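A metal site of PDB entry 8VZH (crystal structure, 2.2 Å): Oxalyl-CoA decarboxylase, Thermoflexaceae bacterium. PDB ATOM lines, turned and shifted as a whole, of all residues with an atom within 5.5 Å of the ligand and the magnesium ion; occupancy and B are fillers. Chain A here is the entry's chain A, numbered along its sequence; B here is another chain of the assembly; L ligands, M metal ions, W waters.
The backbone carbonyl oxygen of Ile 466 lies within hydrogen-bond range of the backbone NH of Asp 441 (3.1 Å). ND1 of His 80 of chain B sits at hydrogen-bond distance from OE1 of Glu 50 of chain B. The backbone carbonyl oxygen (O) of Gly 414 sits at hydrogen-bond distance from the side-chain amide nitrogen (NE2) of Gln 113 of chain B (3.3 Å). The backbone NH (N) of Gly 440 is in hydrogen-bond range of the backbone carbonyl oxygen (O) of Glu 387 (3.1 Å). ND2 of Asn 468 lies within hydrogen-bond range of OH of Tyr 367 (3.0 Å). The side-chain carboxylate (OD2) of Asp 441 lies close to the side-chain amide oxygen (OD1) of Asn 467. The side-chain sulfur (SD) of Met 416 lies close to the backbone NH (N) of Gly 388, at 3.8 Å. The side-chain amide nitrogen (NE2) of Gln 113 of chain B lies within hydrogen-bond range of the backbone carbonyl oxygen (O) of Phe 413, at 3.1 Å.
Of the 37 residues printed, 3 come within 4 Å of the magnesium ion. The nearest printed residue that does not touch the magnesium ion is Gly 472 (4.04 Å).
A nitrogen (N2) of the ligand is in hydrogen-bond range of the backbone NH of Met 416 (3.3 Å). An oxygen (O3) of the ligand sits close to the backbone NH of Ser 442, at 2.9 Å. The backbone NH (N) of Asp 441 lies close to an oxygen (O3) of the ligand (3.1 Å). A nitrogen (N1) of the ligand is in hydrogen-bond range of the side-chain carboxylate (OE2) of Glu 50 of chain B, 2.6 Å away. N of Thr 391 sits at hydrogen-bond distance from O5 of the ligand (3.2 Å). The side-chain hydroxyl (OG1) of Thr 391 is in hydrogen-bond range of an oxygen (O5) of the ligand (2.8 Å). The backbone NH of Gly 472 sits close to an oxygen (O7) of the ligand, at 3.1 Å. The backbone NH of Ser 390 is in hydrogen-bond range of an oxygen (O6) of the ligand. NE2 of Gln 113 of chain B sits close to N3 of the ligand, 3.5 Å away. N of Ala 443 sits at hydrogen-bond distance from O2 of the ligand, 2.9 Å away. The backbone carbonyl oxygen (O) of Gly 414 is in hydrogen-bond range of a nitrogen (N3) of the ligand. The side-chain hydroxyl (OH) of Tyr 367 sits at hydrogen-bond distance from an oxygen (O5) of the ligand, 2.5 Å away.
The magnesium ion is bound by OD1 of Asn 468, 2.1 Å away. The magnesium ion is bound by an oxygen (O3) of the ligand, at 2.1 Å. The magnesium ion is bound by O7 of the ligand. The magnesium ion is bound by OD1 of Asp 441 (2.2 Å). The magnesium ion is bound by the backbone carbonyl oxygen (O) of Gly 470. The magnesium ion is bound by water W1 (2.2 Å). The magnesium ion has six donor atoms within binding distance.
Water W1 lies within hydrogen-bond range of O of Ile 466 (2.6 Å), O5 of the ligand (2.8 Å) and ND2 of Asn 468 (3.4 Å).
Gly 388 touches the ligand. CB of Ala 389 touches O6 of the ligand (3.1 Å). Gly 440 touches the ligand. Phe 446 touches the ligand (CZ to N1, 3.7 Å). Ile 471 touches the ligand. Ile 25 of chain B touches the ligand (CG2 to C10, 3.8 Å). O of Val 26 of chain B touches C10 of the ligand, 3.9 Å away. Val 73 of chain B touches the ligand (CG2 to C5, 3.7 Å). Pro 76 of chain B touches the ligand (C to C2, 3.8 Å). N of Gly 77 of chain B touches C2 of the ligand, 3.7 Å away. His 80 of chain B touches the ligand (CE1 to C2, 3.5 Å). Hydrophobic or aromatic side chains within 4 Å of the ligand: Tyr 367, Ala 389, Met 416, Ala 443, Phe 446, Ile 471, Ile 25 of chain B, Val 73 of chain B, Pro 76 of chain B and His 80 of chain B. Of the 37 residues printed, 24 come within 4 Å of the ligand.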
ATOM      1  N   TYR A 367      17.290  11.440  19.340  1.00  0.00           N
ATOM      2  CA  TYR A 367      16.100  12.291  19.409  1.00  0.00           C
ATOM      3  C   TYR A 367      16.398  13.698  18.891  1.00  0.00           C
ATOM      4  O   TYR A 367      15.631  14.249  18.080  1.00  0.00           O
ATOM      5  CB  TYR A 367      15.594  12.363  20.845  1.00  0.00           C
ATOM      6  CG  TYR A 367      14.892  11.114  21.350  1.00  0.00           C
ATOM      7  CD1 TYR A 367      13.544  10.901  21.086  1.00  0.00           C
ATOM      8  CD2 TYR A 367      15.571  10.174  22.111  1.00  0.00           C
ATOM      9  CE1 TYR A 367      12.895   9.773  21.567  1.00  0.00           C
ATOM     10  CE2 TYR A 367      14.935   9.050  22.597  1.00  0.00           C
ATOM     11  CZ  TYR A 367      13.603   8.853  22.316  1.00  0.00           C
ATOM     12  OH  TYR A 367      12.963   7.733  22.789  1.00  0.00           O
ATOM     13  N   GLU A 387       3.361  12.963  22.114  1.00  0.00           N
ATOM     14  CA  GLU A 387       2.940  11.923  23.042  1.00  0.00           C
ATOM     15  C   GLU A 387       3.981  10.827  23.133  1.00  0.00           C
ATOM     16  O   GLU A 387       4.552  10.411  22.122  1.00  0.00           O
ATOM     17  CB  GLU A 387       1.591  11.313  22.613  1.00  0.00           C
ATOM     18  CG  GLU A 387       1.025  10.306  23.597  1.00  0.00           C
ATOM     19  CD  GLU A 387      -0.137   9.505  23.028  1.00  0.00           C
ATOM     20  OE1 GLU A 387      -0.188   9.309  21.784  1.00  0.00           O
ATOM     21  OE2 GLU A 387      -1.005   9.060  23.811  1.00  0.00           O
ATOM     22  N   GLY A 388       4.202  10.326  24.340  1.00  0.00           N
ATOM     23  CA  GLY A 388       5.203   9.295  24.538  1.00  0.00           C
ATOM     24  C   GLY A 388       5.962   9.539  25.826  1.00  0.00           C
ATOM     25  O   GLY A 388       5.438  10.178  26.735  1.00  0.00           O
ATOM     26  N   ALA A 389       7.184   9.026  25.919  1.00  0.00           N
ATOM     27  CA  ALA A 389       7.987   9.281  27.105  1.00  0.00           C
ATOM     28  C   ALA A 389       9.104  10.215  26.691  1.00  0.00           C
ATOM     29  O   ALA A 389       8.924  11.453  26.742  1.00  0.00           O
ATOM     30  CB  ALA A 389       8.471   7.968  27.748  1.00  0.00           C
ATOM     31  N   SER A 390      10.258   9.711  26.241  1.00  0.00           N
ATOM     32  CA  SER A 390      11.319  10.610  25.774  1.00  0.00           C
ATOM     33  C   SER A 390      10.879  11.390  24.543  1.00  0.00           C
ATOM     34  O   SER A 390      11.221  12.569  24.395  1.00  0.00           O
ATOM     35  CB  SER A 390      12.590   9.830  25.492  1.00  0.00           C
ATOM     36  OG  SER A 390      13.123   9.278  26.684  1.00  0.00           O
ATOM     37  N   THR A 391      10.129  10.755  23.639  1.00  0.00           N
ATOM     38  CA  THR A 391       9.606  11.468  22.478  1.00  0.00           C
ATOM     39  C   THR A 391       8.846  12.733  22.891  1.00  0.00           C
ATOM     40  O   THR A 391       8.974  13.787  22.252  1.00  0.00           O
ATOM     41  CB  THR A 391       8.704  10.553  21.649  1.00  0.00           C
ATOM     42  OG1 THR A 391       9.481   9.485  21.091  1.00  0.00           O
ATOM     43  CG2 THR A 391       8.037  11.323  20.519  1.00  0.00           C
ATOM     44  N   PHE A 413      -2.501  13.584  33.621  1.00  0.00           N
ATOM     45  CA  PHE A 413      -2.678  12.157  33.865  1.00  0.00           C
ATOM     46  C   PHE A 413      -1.581  11.308  33.222  1.00  0.00           C
ATOM     47  O   PHE A 413      -1.575  10.097  33.433  1.00  0.00           O
ATOM     48  CB  PHE A 413      -4.045  11.700  33.336  1.00  0.00           C
ATOM     49  CG  PHE A 413      -4.788  10.775  34.268  1.00  0.00           C
ATOM     50  CD1 PHE A 413      -4.467  10.715  35.611  1.00  0.00           C
ATOM     51  CD2 PHE A 413      -5.811   9.964  33.781  1.00  0.00           C
ATOM     52  CE1 PHE A 413      -5.152   9.871  36.461  1.00  0.00           C
ATOM     53  CE2 PHE A 413      -6.503   9.123  34.627  1.00  0.00           C
ATOM     54  CZ  PHE A 413      -6.170   9.068  35.975  1.00  0.00           C
ATOM     55  N   GLY A 414      -0.675  11.901  32.450  1.00  0.00           N
ATOM     56  CA  GLY A 414       0.347  11.115  31.779  1.00  0.00           C
ATOM     57  C   GLY A 414      -0.207  10.010  30.911  1.00  0.00           C
ATOM     58  O   GLY A 414       0.349   8.908  30.874  1.00  0.00           O
ATOM     59  N   THR A 415      -1.297  10.285  30.201  1.00  0.00           N
ATOM     60  CA  THR A 415      -2.037   9.255  29.497  1.00  0.00           C
ATOM     61  C   THR A 415      -1.387   8.935  28.149  1.00  0.00           C
ATOM     62  O   THR A 415      -1.187   9.826  27.329  1.00  0.00           O
ATOM     63  CB  THR A 415      -3.471   9.719  29.276  1.00  0.00           C
ATOM     64  OG1 THR A 415      -4.003  10.205  30.515  1.00  0.00           O
ATOM     65  CG2 THR A 415      -4.331   8.584  28.752  1.00  0.00           C
ATOM     66  N   MET A 416      -1.086   7.654  27.925  1.00  0.00           N
ATOM     67  CA  MET A 416      -0.847   7.155  26.585  1.00  0.00           C
ATOM     68  C   MET A 416      -2.187   6.773  25.960  1.00  0.00           C
ATOM     69  O   MET A 416      -3.053   6.205  26.627  1.00  0.00           O
ATOM     70  CB  MET A 416       0.087   5.942  26.589  1.00  0.00           C
ATOM     71  CG  MET A 416       1.510   6.235  27.018  1.00  0.00           C
ATOM     72  SD  MET A 416       2.305   7.491  25.995  1.00  0.00           S
ATOM     73  CE  MET A 416       2.217   8.939  27.067  1.00  0.00           C
ATOM     74  N   GLN A 439       4.678  11.077  17.900  1.00  0.00           N
ATOM     75  CA  GLN A 439       4.522  10.065  18.927  1.00  0.00           C
ATOM     76  C   GLN A 439       5.706   9.118  18.942  1.00  0.00           C
ATOM     77  O   GLN A 439       6.340   8.864  17.906  1.00  0.00           O
ATOM     78  CB  GLN A 439       3.259   9.234  18.711  1.00  0.00           C
ATOM     79  CG  GLN A 439       1.983  10.028  18.663  1.00  0.00           C
ATOM     80  CD  GLN A 439       0.832   9.177  18.191  1.00  0.00           C
ATOM     81  OE1 GLN A 439       0.010   8.732  18.983  1.00  0.00           O
ATOM     82  NE2 GLN A 439       0.783   8.930  16.888  1.00  0.00           N
ATOM     83  N   GLY A 440       5.990   8.577  20.125  1.00  0.00           N
ATOM     84  CA  GLY A 440       6.832   7.401  20.206  1.00  0.00           C
ATOM     85  C   GLY A 440       6.117   6.175  19.666  1.00  0.00           C
ATOM     86  O   GLY A 440       4.887   6.146  19.541  1.00  0.00           O
ATOM     87  N   ASP A 441       6.899   5.149  19.323  1.00  0.00           N
ATOM     88  CA  ASP A 441       6.289   3.981  18.679  1.00  0.00           C
ATOM     89  C   ASP A 441       5.233   3.338  19.578  1.00  0.00           C
ATOM     90  O   ASP A 441       4.153   2.979  19.105  1.00  0.00           O
ATOM     91  CB  ASP A 441       7.365   2.962  18.274  1.00  0.00           C
ATOM     92  CG  ASP A 441       8.287   2.558  19.418  1.00  0.00           C
ATOM     93  OD1 ASP A 441       8.906   3.442  20.053  1.00  0.00           O
ATOM     94  OD2 ASP A 441       8.411   1.340  19.658  1.00  0.00           O
ATOM     95  N   SER A 442       5.515   3.235  20.877  1.00  0.00           N
ATOM     96  CA  SER A 442       4.519   2.672  21.793  1.00  0.00           C
ATOM     97  C   SER A 442       3.259   3.528  21.832  1.00  0.00           C
ATOM     98  O   SER A 442       2.136   3.016  21.761  1.00  0.00           O
ATOM     99  CB  SER A 442       5.107   2.519  23.194  1.00  0.00           C
ATOM    100  OG  SER A 442       4.163   1.947  24.068  1.00  0.00           O
ATOM    101  N   ALA A 443       3.439   4.848  21.972  1.00  0.00           N
ATOM    102  CA  ALA A 443       2.287   5.752  21.997  1.00  0.00           C
ATOM    103  C   ALA A 443       1.441   5.569  20.752  1.00  0.00           C
ATOM    104  O   ALA A 443       0.207   5.533  20.834  1.00  0.00           O
ATOM    105  CB  ALA A 443       2.762   7.208  22.116  1.00  0.00           C
ATOM    106  N   PHE A 444       2.080   5.437  19.586  1.00  0.00           N
ATOM    107  CA  PHE A 444       1.318   5.311  18.360  1.00  0.00           C
ATOM    108  C   PHE A 444       0.412   4.089  18.371  1.00  0.00           C
ATOM    109  O   PHE A 444      -0.672   4.115  17.778  1.00  0.00           O
ATOM    110  CB  PHE A 444       2.250   5.264  17.144  1.00  0.00           C
ATOM    111  CG  PHE A 444       1.543   5.004  15.858  1.00  0.00           C
ATOM    112  CD1 PHE A 444       0.848   6.019  15.213  1.00  0.00           C
ATOM    113  CD2 PHE A 444       1.532   3.733  15.293  1.00  0.00           C
ATOM    114  CE1 PHE A 444       0.172   5.790  14.024  1.00  0.00           C
ATOM    115  CE2 PHE A 444       0.855   3.482  14.106  1.00  0.00           C
ATOM    116  CZ  PHE A 444       0.174   4.511  13.476  1.00  0.00           C
ATOM    117  N   PHE A 446      -1.319   2.768  20.750  1.00  0.00           N
ATOM    118  CA  PHE A 446      -2.511   2.835  21.602  1.00  0.00           C
ATOM    119  C   PHE A 446      -3.755   3.185  20.808  1.00  0.00           C
ATOM    120  O   PHE A 446      -4.858   2.763  21.183  1.00  0.00           O
ATOM    121  CB  PHE A 446      -2.315   3.847  22.721  1.00  0.00           C
ATOM    122  CG  PHE A 446      -1.581   3.296  23.911  1.00  0.00           C
ATOM    123  CD1 PHE A 446      -0.206   3.156  23.876  1.00  0.00           C
ATOM    124  CD2 PHE A 446      -2.277   2.920  25.054  1.00  0.00           C
ATOM    125  CE1 PHE A 446       0.474   2.652  24.972  1.00  0.00           C
ATOM    126  CE2 PHE A 446      -1.596   2.416  26.150  1.00  0.00           C
ATOM    127  CZ  PHE A 446      -0.225   2.289  26.112  1.00  0.00           C
ATOM    128  N   ILE A 466       8.397   8.209  16.186  1.00  0.00           N
ATOM    129  CA  ILE A 466       9.803   8.147  16.559  1.00  0.00           C
ATOM    130  C   ILE A 466      10.008   6.801  17.229  1.00  0.00           C
ATOM    131  O   ILE A 466       9.509   6.554  18.344  1.00  0.00           O
ATOM    132  CB  ILE A 466      10.201   9.327  17.451  1.00  0.00           C
ATOM    133  CG1 ILE A 466      10.166  10.616  16.619  1.00  0.00           C
ATOM    134  CG2 ILE A 466      11.560   9.084  18.075  1.00  0.00           C
ATOM    135  CD1 ILE A 466      10.556  11.861  17.369  1.00  0.00           C
ATOM    136  N   ASN A 467      10.728   5.895  16.563  1.00  0.00           N
ATOM    137  CA  ASN A 467      10.607   4.464  16.788  1.00  0.00           C
ATOM    138  C   ASN A 467      11.940   3.902  17.261  1.00  0.00           C
ATOM    139  O   ASN A 467      12.876   3.754  16.462  1.00  0.00           O
ATOM    140  CB  ASN A 467      10.130   3.788  15.502  1.00  0.00           C
ATOM    141  CG  ASN A 467       9.807   2.316  15.690  1.00  0.00           C
ATOM    142  OD1 ASN A 467      10.107   1.715  16.723  1.00  0.00           O
ATOM    143  ND2 ASN A 467       9.207   1.709  14.661  1.00  0.00           N
ATOM    144  N   ASN A 468      12.025   3.572  18.556  1.00  0.00           N
ATOM    145  CA  ASN A 468      13.188   2.893  19.122  1.00  0.00           C
ATOM    146  C   ASN A 468      12.893   1.435  19.472  1.00  0.00           C
ATOM    147  O   ASN A 468      13.622   0.825  20.273  1.00  0.00           O
ATOM    148  CB  ASN A 468      13.720   3.638  20.347  1.00  0.00           C
ATOM    149  CG  ASN A 468      12.645   3.920  21.378  1.00  0.00           C
ATOM    150  OD1 ASN A 468      11.538   3.377  21.317  1.00  0.00           O
ATOM    151  ND2 ASN A 468      12.964   4.774  22.348  1.00  0.00           N
ATOM    152  N   ASN A 469      11.821   0.870  18.905  1.00  0.00           N
ATOM    153  CA  ASN A 469      11.438  -0.534  19.037  1.00  0.00           C
ATOM    154  C   ASN A 469      10.821  -0.880  20.386  1.00  0.00           C
ATOM    155  O   ASN A 469      10.848  -2.043  20.786  1.00  0.00           O
ATOM    156  CB  ASN A 469      12.616  -1.496  18.790  1.00  0.00           C
ATOM    157  CG  ASN A 469      13.063  -1.504  17.343  1.00  0.00           C
ATOM    158  OD1 ASN A 469      12.311  -1.164  16.442  1.00  0.00           O
ATOM    159  ND2 ASN A 469      14.311  -1.910  17.119  1.00  0.00           N
ATOM    160  N   GLY A 470      10.264   0.084  21.114  1.00  0.00           N
ATOM    161  CA  GLY A 470       9.538  -0.281  22.309  1.00  0.00           C
ATOM    162  C   GLY A 470       9.324   0.894  23.258  1.00  0.00           C
ATOM    163  O   GLY A 470       9.465   2.062  22.874  1.00  0.00           O
ATOM    164  N   ILE A 471       8.957   0.537  24.484  1.00  0.00           N
ATOM    165  CA  ILE A 471       8.680   1.484  25.563  1.00  0.00           C
ATOM    166  C   ILE A 471      10.037   1.872  26.161  1.00  0.00           C
ATOM    167  O   ILE A 471      10.625   1.111  26.929  1.00  0.00           O
ATOM    168  CB  ILE A 471       7.747   0.888  26.618  1.00  0.00           C
ATOM    169  CG1 ILE A 471       6.398   0.523  25.978  1.00  0.00           C
ATOM    170  CG2 ILE A 471       7.541   1.848  27.769  1.00  0.00           C
ATOM    171  CD1 ILE A 471       5.480  -0.268  26.886  1.00  0.00           C
ATOM    172  N   GLY A 472      10.530   3.053  25.805  1.00  0.00           N
ATOM    173  CA  GLY A 472      11.890   3.396  26.168  1.00  0.00           C
ATOM    174  C   GLY A 472      12.939   2.628  25.409  1.00  0.00           C
ATOM    175  O   GLY A 472      14.112   2.682  25.780  1.00  0.00           O
ATOM    176  N   GLY A 473      12.551   1.915  24.383  1.00  0.00           N
ATOM    177  CA  GLY A 473      13.513   1.232  23.544  1.00  0.00           C
ATOM    178  C   GLY A 473      13.366  -0.268  23.591  1.00  0.00           C
ATOM    179  O   GLY A 473      12.975  -0.851  24.613  1.00  0.00           O
ATOM    180  N   ILE A 534      15.169   5.417  15.484  1.00  0.00           N
ATOM    181  CA  ILE A 534      16.195   6.036  16.310  1.00  0.00           C
ATOM    182  C   ILE A 534      16.854   4.951  17.155  1.00  0.00           C
ATOM    183  O   ILE A 534      16.358   3.829  17.274  1.00  0.00           O
ATOM    184  CB  ILE A 534      15.643   7.172  17.197  1.00  0.00           C
ATOM    185  CG1 ILE A 534      14.476   6.657  18.035  1.00  0.00           C
ATOM    186  CG2 ILE A 534      15.229   8.370  16.356  1.00  0.00           C
ATOM    187  CD1 ILE A 534      14.408   7.257  19.415  1.00  0.00           C
ATOM    188  N   ILE B  25       0.562  -3.705  29.892  1.00  0.00           N
ATOM    189  CA  ILE B  25       1.537  -2.777  29.353  1.00  0.00           C
ATOM    190  C   ILE B  25       2.346  -2.232  30.521  1.00  0.00           C
ATOM    191  O   ILE B  25       1.777  -1.734  31.492  1.00  0.00           O
ATOM    192  CB  ILE B  25       0.869  -1.638  28.564  1.00  0.00           C
ATOM    193  CG1 ILE B  25       0.039  -2.209  27.412  1.00  0.00           C
ATOM    194  CG2 ILE B  25       1.912  -0.647  28.058  1.00  0.00           C
ATOM    195  CD1 ILE B  25      -0.639  -1.170  26.554  1.00  0.00           C
ATOM    196  N   VAL B  26       3.677  -2.332  30.419  1.00  0.00           N
ATOM    197  CA  VAL B  26       4.523  -1.980  31.546  1.00  0.00           C
ATOM    198  C   VAL B  26       4.714  -0.469  31.626  1.00  0.00           C
ATOM    199  O   VAL B  26       4.494   0.275  30.666  1.00  0.00           O
ATOM    200  CB  VAL B  26       5.890  -2.694  31.472  1.00  0.00           C
ATOM    201  CG1 VAL B  26       5.713  -4.194  31.658  1.00  0.00           C
ATOM    202  CG2 VAL B  26       6.580  -2.365  30.157  1.00  0.00           C
ATOM    203  N   GLY B  27       5.176  -0.029  32.778  1.00  0.00           N
ATOM    204  CA  GLY B  27       5.322   1.367  33.103  1.00  0.00           C
ATOM    205  C   GLY B  27       5.302   1.528  34.605  1.00  0.00           C
ATOM    206  O   GLY B  27       4.952   0.607  35.343  1.00  0.00           O
ATOM    207  N   ILE B  28       5.720   2.710  35.046  1.00  0.00           N
ATOM    208  CA  ILE B  28       5.696   3.026  36.475  1.00  0.00           C
ATOM    209  C   ILE B  28       4.288   2.774  37.009  1.00  0.00           C
ATOM    210  O   ILE B  28       3.314   3.269  36.433  1.00  0.00           O
ATOM    211  CB  ILE B  28       6.113   4.487  36.722  1.00  0.00           C
ATOM    212  CG1 ILE B  28       7.451   4.777  36.046  1.00  0.00           C
ATOM    213  CG2 ILE B  28       6.179   4.774  38.214  1.00  0.00           C
ATOM    214  CD1 ILE B  28       7.889   6.219  36.150  1.00  0.00           C
ATOM    215  N   GLU B  50      -4.271  -1.429  27.073  1.00  0.00           N
ATOM    216  CA  GLU B  50      -4.737  -2.241  28.198  1.00  0.00           C
ATOM    217  C   GLU B  50      -6.166  -2.713  28.015  1.00  0.00           C
ATOM    218  O   GLU B  50      -6.566  -3.710  28.641  1.00  0.00           O
ATOM    219  CB  GLU B  50      -4.648  -1.477  29.516  1.00  0.00           C
ATOM    220  CG  GLU B  50      -3.254  -1.100  29.924  1.00  0.00           C
ATOM    221  CD  GLU B  50      -2.806   0.208  29.317  1.00  0.00           C
ATOM    222  OE1 GLU B  50      -3.568   0.778  28.517  1.00  0.00           O
ATOM    223  OE2 GLU B  50      -1.697   0.655  29.650  1.00  0.00           O
ATOM    224  N   VAL B  73      -0.666   0.084  34.581  1.00  0.00           N
ATOM    225  CA  VAL B  73      -0.038   1.163  35.341  1.00  0.00           C
ATOM    226  C   VAL B  73      -1.104   1.928  36.105  1.00  0.00           C
ATOM    227  O   VAL B  73      -2.303   1.710  35.937  1.00  0.00           O
ATOM    228  CB  VAL B  73       0.752   2.120  34.425  1.00  0.00           C
ATOM    229  CG1 VAL B  73       1.780   1.356  33.612  1.00  0.00           C
ATOM    230  CG2 VAL B  73      -0.201   2.907  33.521  1.00  0.00           C
ATOM    231  N   PRO B  76      -4.601   6.164  34.293  1.00  0.00           N
ATOM    232  CA  PRO B  76      -5.250   5.818  33.019  1.00  0.00           C
ATOM    233  C   PRO B  76      -5.036   4.377  32.590  1.00  0.00           C
ATOM    234  O   PRO B  76      -5.861   3.829  31.863  1.00  0.00           O
ATOM    235  CB  PRO B  76      -4.628   6.809  32.028  1.00  0.00           C
ATOM    236  CG  PRO B  76      -3.305   7.158  32.627  1.00  0.00           C
ATOM    237  CD  PRO B  76      -3.523   7.149  34.118  1.00  0.00           C
ATOM    238  N   GLY B  77      -3.931   3.742  33.018  1.00  0.00           N
ATOM    239  CA  GLY B  77      -3.722   2.352  32.657  1.00  0.00           C
ATOM    240  C   GLY B  77      -4.752   1.441  33.302  1.00  0.00           C
ATOM    241  O   GLY B  77      -5.346   0.594  32.630  1.00  0.00           O
ATOM    242  N   HIS B  80      -8.301   2.117  31.605  1.00  0.00           N
ATOM    243  CA  HIS B  80      -8.447   1.302  30.399  1.00  0.00           C
ATOM    244  C   HIS B  80      -8.795  -0.151  30.737  1.00  0.00           C
ATOM    245  O   HIS B  80      -9.547  -0.802  29.998  1.00  0.00           O
ATOM    246  CB  HIS B  80      -7.153   1.338  29.579  1.00  0.00           C
ATOM    247  CG  HIS B  80      -6.833   2.684  29.000  1.00  0.00           C
ATOM    248  ND1 HIS B  80      -5.712   2.911  28.239  1.00  0.00           N
ATOM    249  CD2 HIS B  80      -7.489   3.864  29.074  1.00  0.00           C
ATOM    250  CE1 HIS B  80      -5.689   4.182  27.859  1.00  0.00           C
ATOM    251  NE2 HIS B  80      -6.754   4.782  28.358  1.00  0.00           N
ATOM    252  N   PHE B 112       1.680  11.625  40.605  1.00  0.00           N
ATOM    253  CA  PHE B 112       1.597  11.166  39.234  1.00  0.00           C
ATOM    254  C   PHE B 112       0.570  10.039  39.118  1.00  0.00           C
ATOM    255  O   PHE B 112       0.692   8.995  39.763  1.00  0.00           O
ATOM    256  CB  PHE B 112       2.969  10.701  38.763  1.00  0.00           C
ATOM    257  CG  PHE B 112       2.992  10.229  37.340  1.00  0.00           C
ATOM    258  CD1 PHE B 112       2.723  11.116  36.310  1.00  0.00           C
ATOM    259  CD2 PHE B 112       3.274   8.910  37.035  1.00  0.00           C
ATOM    260  CE1 PHE B 112       2.740  10.691  35.000  1.00  0.00           C
ATOM    261  CE2 PHE B 112       3.300   8.480  35.729  1.00  0.00           C
ATOM    262  CZ  PHE B 112       3.027   9.368  34.709  1.00  0.00           C
ATOM    263  N   GLN B 113      -0.465  10.286  38.314  1.00  0.00           N
ATOM    264  CA  GLN B 113      -1.519   9.299  38.051  1.00  0.00           C
ATOM    265  C   GLN B 113      -2.266   8.892  39.318  1.00  0.00           C
ATOM    266  O   GLN B 113      -2.754   7.755  39.432  1.00  0.00           O
ATOM    267  CB  GLN B 113      -0.946   8.094  37.301  1.00  0.00           C
ATOM    268  CG  GLN B 113      -0.480   8.486  35.906  1.00  0.00           C
ATOM    269  CD  GLN B 113       0.119   7.349  35.126  1.00  0.00           C
ATOM    270  OE1 GLN B 113       0.559   6.355  35.705  1.00  0.00           O
ATOM    271  NE2 GLN B 113       0.136   7.485  33.809  1.00  0.00           N
HETATM  272  N1  LIG L   1      -0.612   3.055  29.750  1.00  0.00           N
HETATM  273  C1  LIG L   1      -1.171   4.272  29.872  1.00  0.00           C
HETATM  274  C2  LIG L   1      -2.630   4.393  29.623  1.00  0.00           C
HETATM  275  N2  LIG L   1      -0.508   5.390  30.195  1.00  0.00           N
HETATM  276  C3  LIG L   1       0.817   5.304  30.427  1.00  0.00           C
HETATM  277  N3  LIG L   1       1.447   6.427  30.747  1.00  0.00           N
HETATM  278  C4  LIG L   1       1.497   4.048  30.318  1.00  0.00           C
HETATM  279  C5  LIG L   1       0.697   2.978  29.975  1.00  0.00           C
HETATM  280  C6  LIG L   1       2.967   3.890  30.553  1.00  0.00           C
HETATM  281  N4  LIG L   1       3.799   4.608  29.562  1.00  0.00           N
HETATM  282  C7  LIG L   1       4.356   5.778  29.779  1.00  0.00           C
HETATM  283  S1  LIG L   1       5.222   6.334  28.459  1.00  0.00           S
HETATM  284  C8  LIG L   1       4.824   4.919  27.561  1.00  0.00           C
HETATM  285  C9  LIG L   1       4.043   4.089  28.292  1.00  0.00           C
HETATM  286  C10 LIG L   1       3.490   2.769  27.874  1.00  0.00           C
HETATM  287  C11 LIG L   1       5.323   4.747  26.154  1.00  0.00           C
HETATM  288  C12 LIG L   1       6.798   5.061  26.013  1.00  0.00           C
HETATM  289  O1  LIG L   1       7.252   4.586  24.718  1.00  0.00           O
HETATM  290  P1  LIG L   1       7.193   5.443  23.399  1.00  0.00           P
HETATM  291  O2  LIG L   1       5.840   6.002  23.169  1.00  0.00           O
HETATM  292  O3  LIG L   1       7.722   4.602  22.252  1.00  0.00           O
HETATM  293  O4  LIG L   1       8.287   6.515  23.724  1.00  0.00           O
HETATM  294  P2  LIG L   1       9.862   6.618  23.856  1.00  0.00           P
HETATM  295  O5  LIG L   1      10.420   7.615  22.903  1.00  0.00           O
HETATM  296  O6  LIG L   1      10.108   6.919  25.325  1.00  0.00           O
HETATM  297  O7  LIG L   1      10.345   5.174  23.585  1.00  0.00           O
HETATM  298 MG    MG M   1       9.698   4.032  21.973  1.00  0.00          MG
HETATM  299  O   HOH W   1      10.170   5.836  20.776  1.00  0.00           O
HETATM  300  O   HOH W   2       4.076   6.624  32.876  1.00  0.00           O
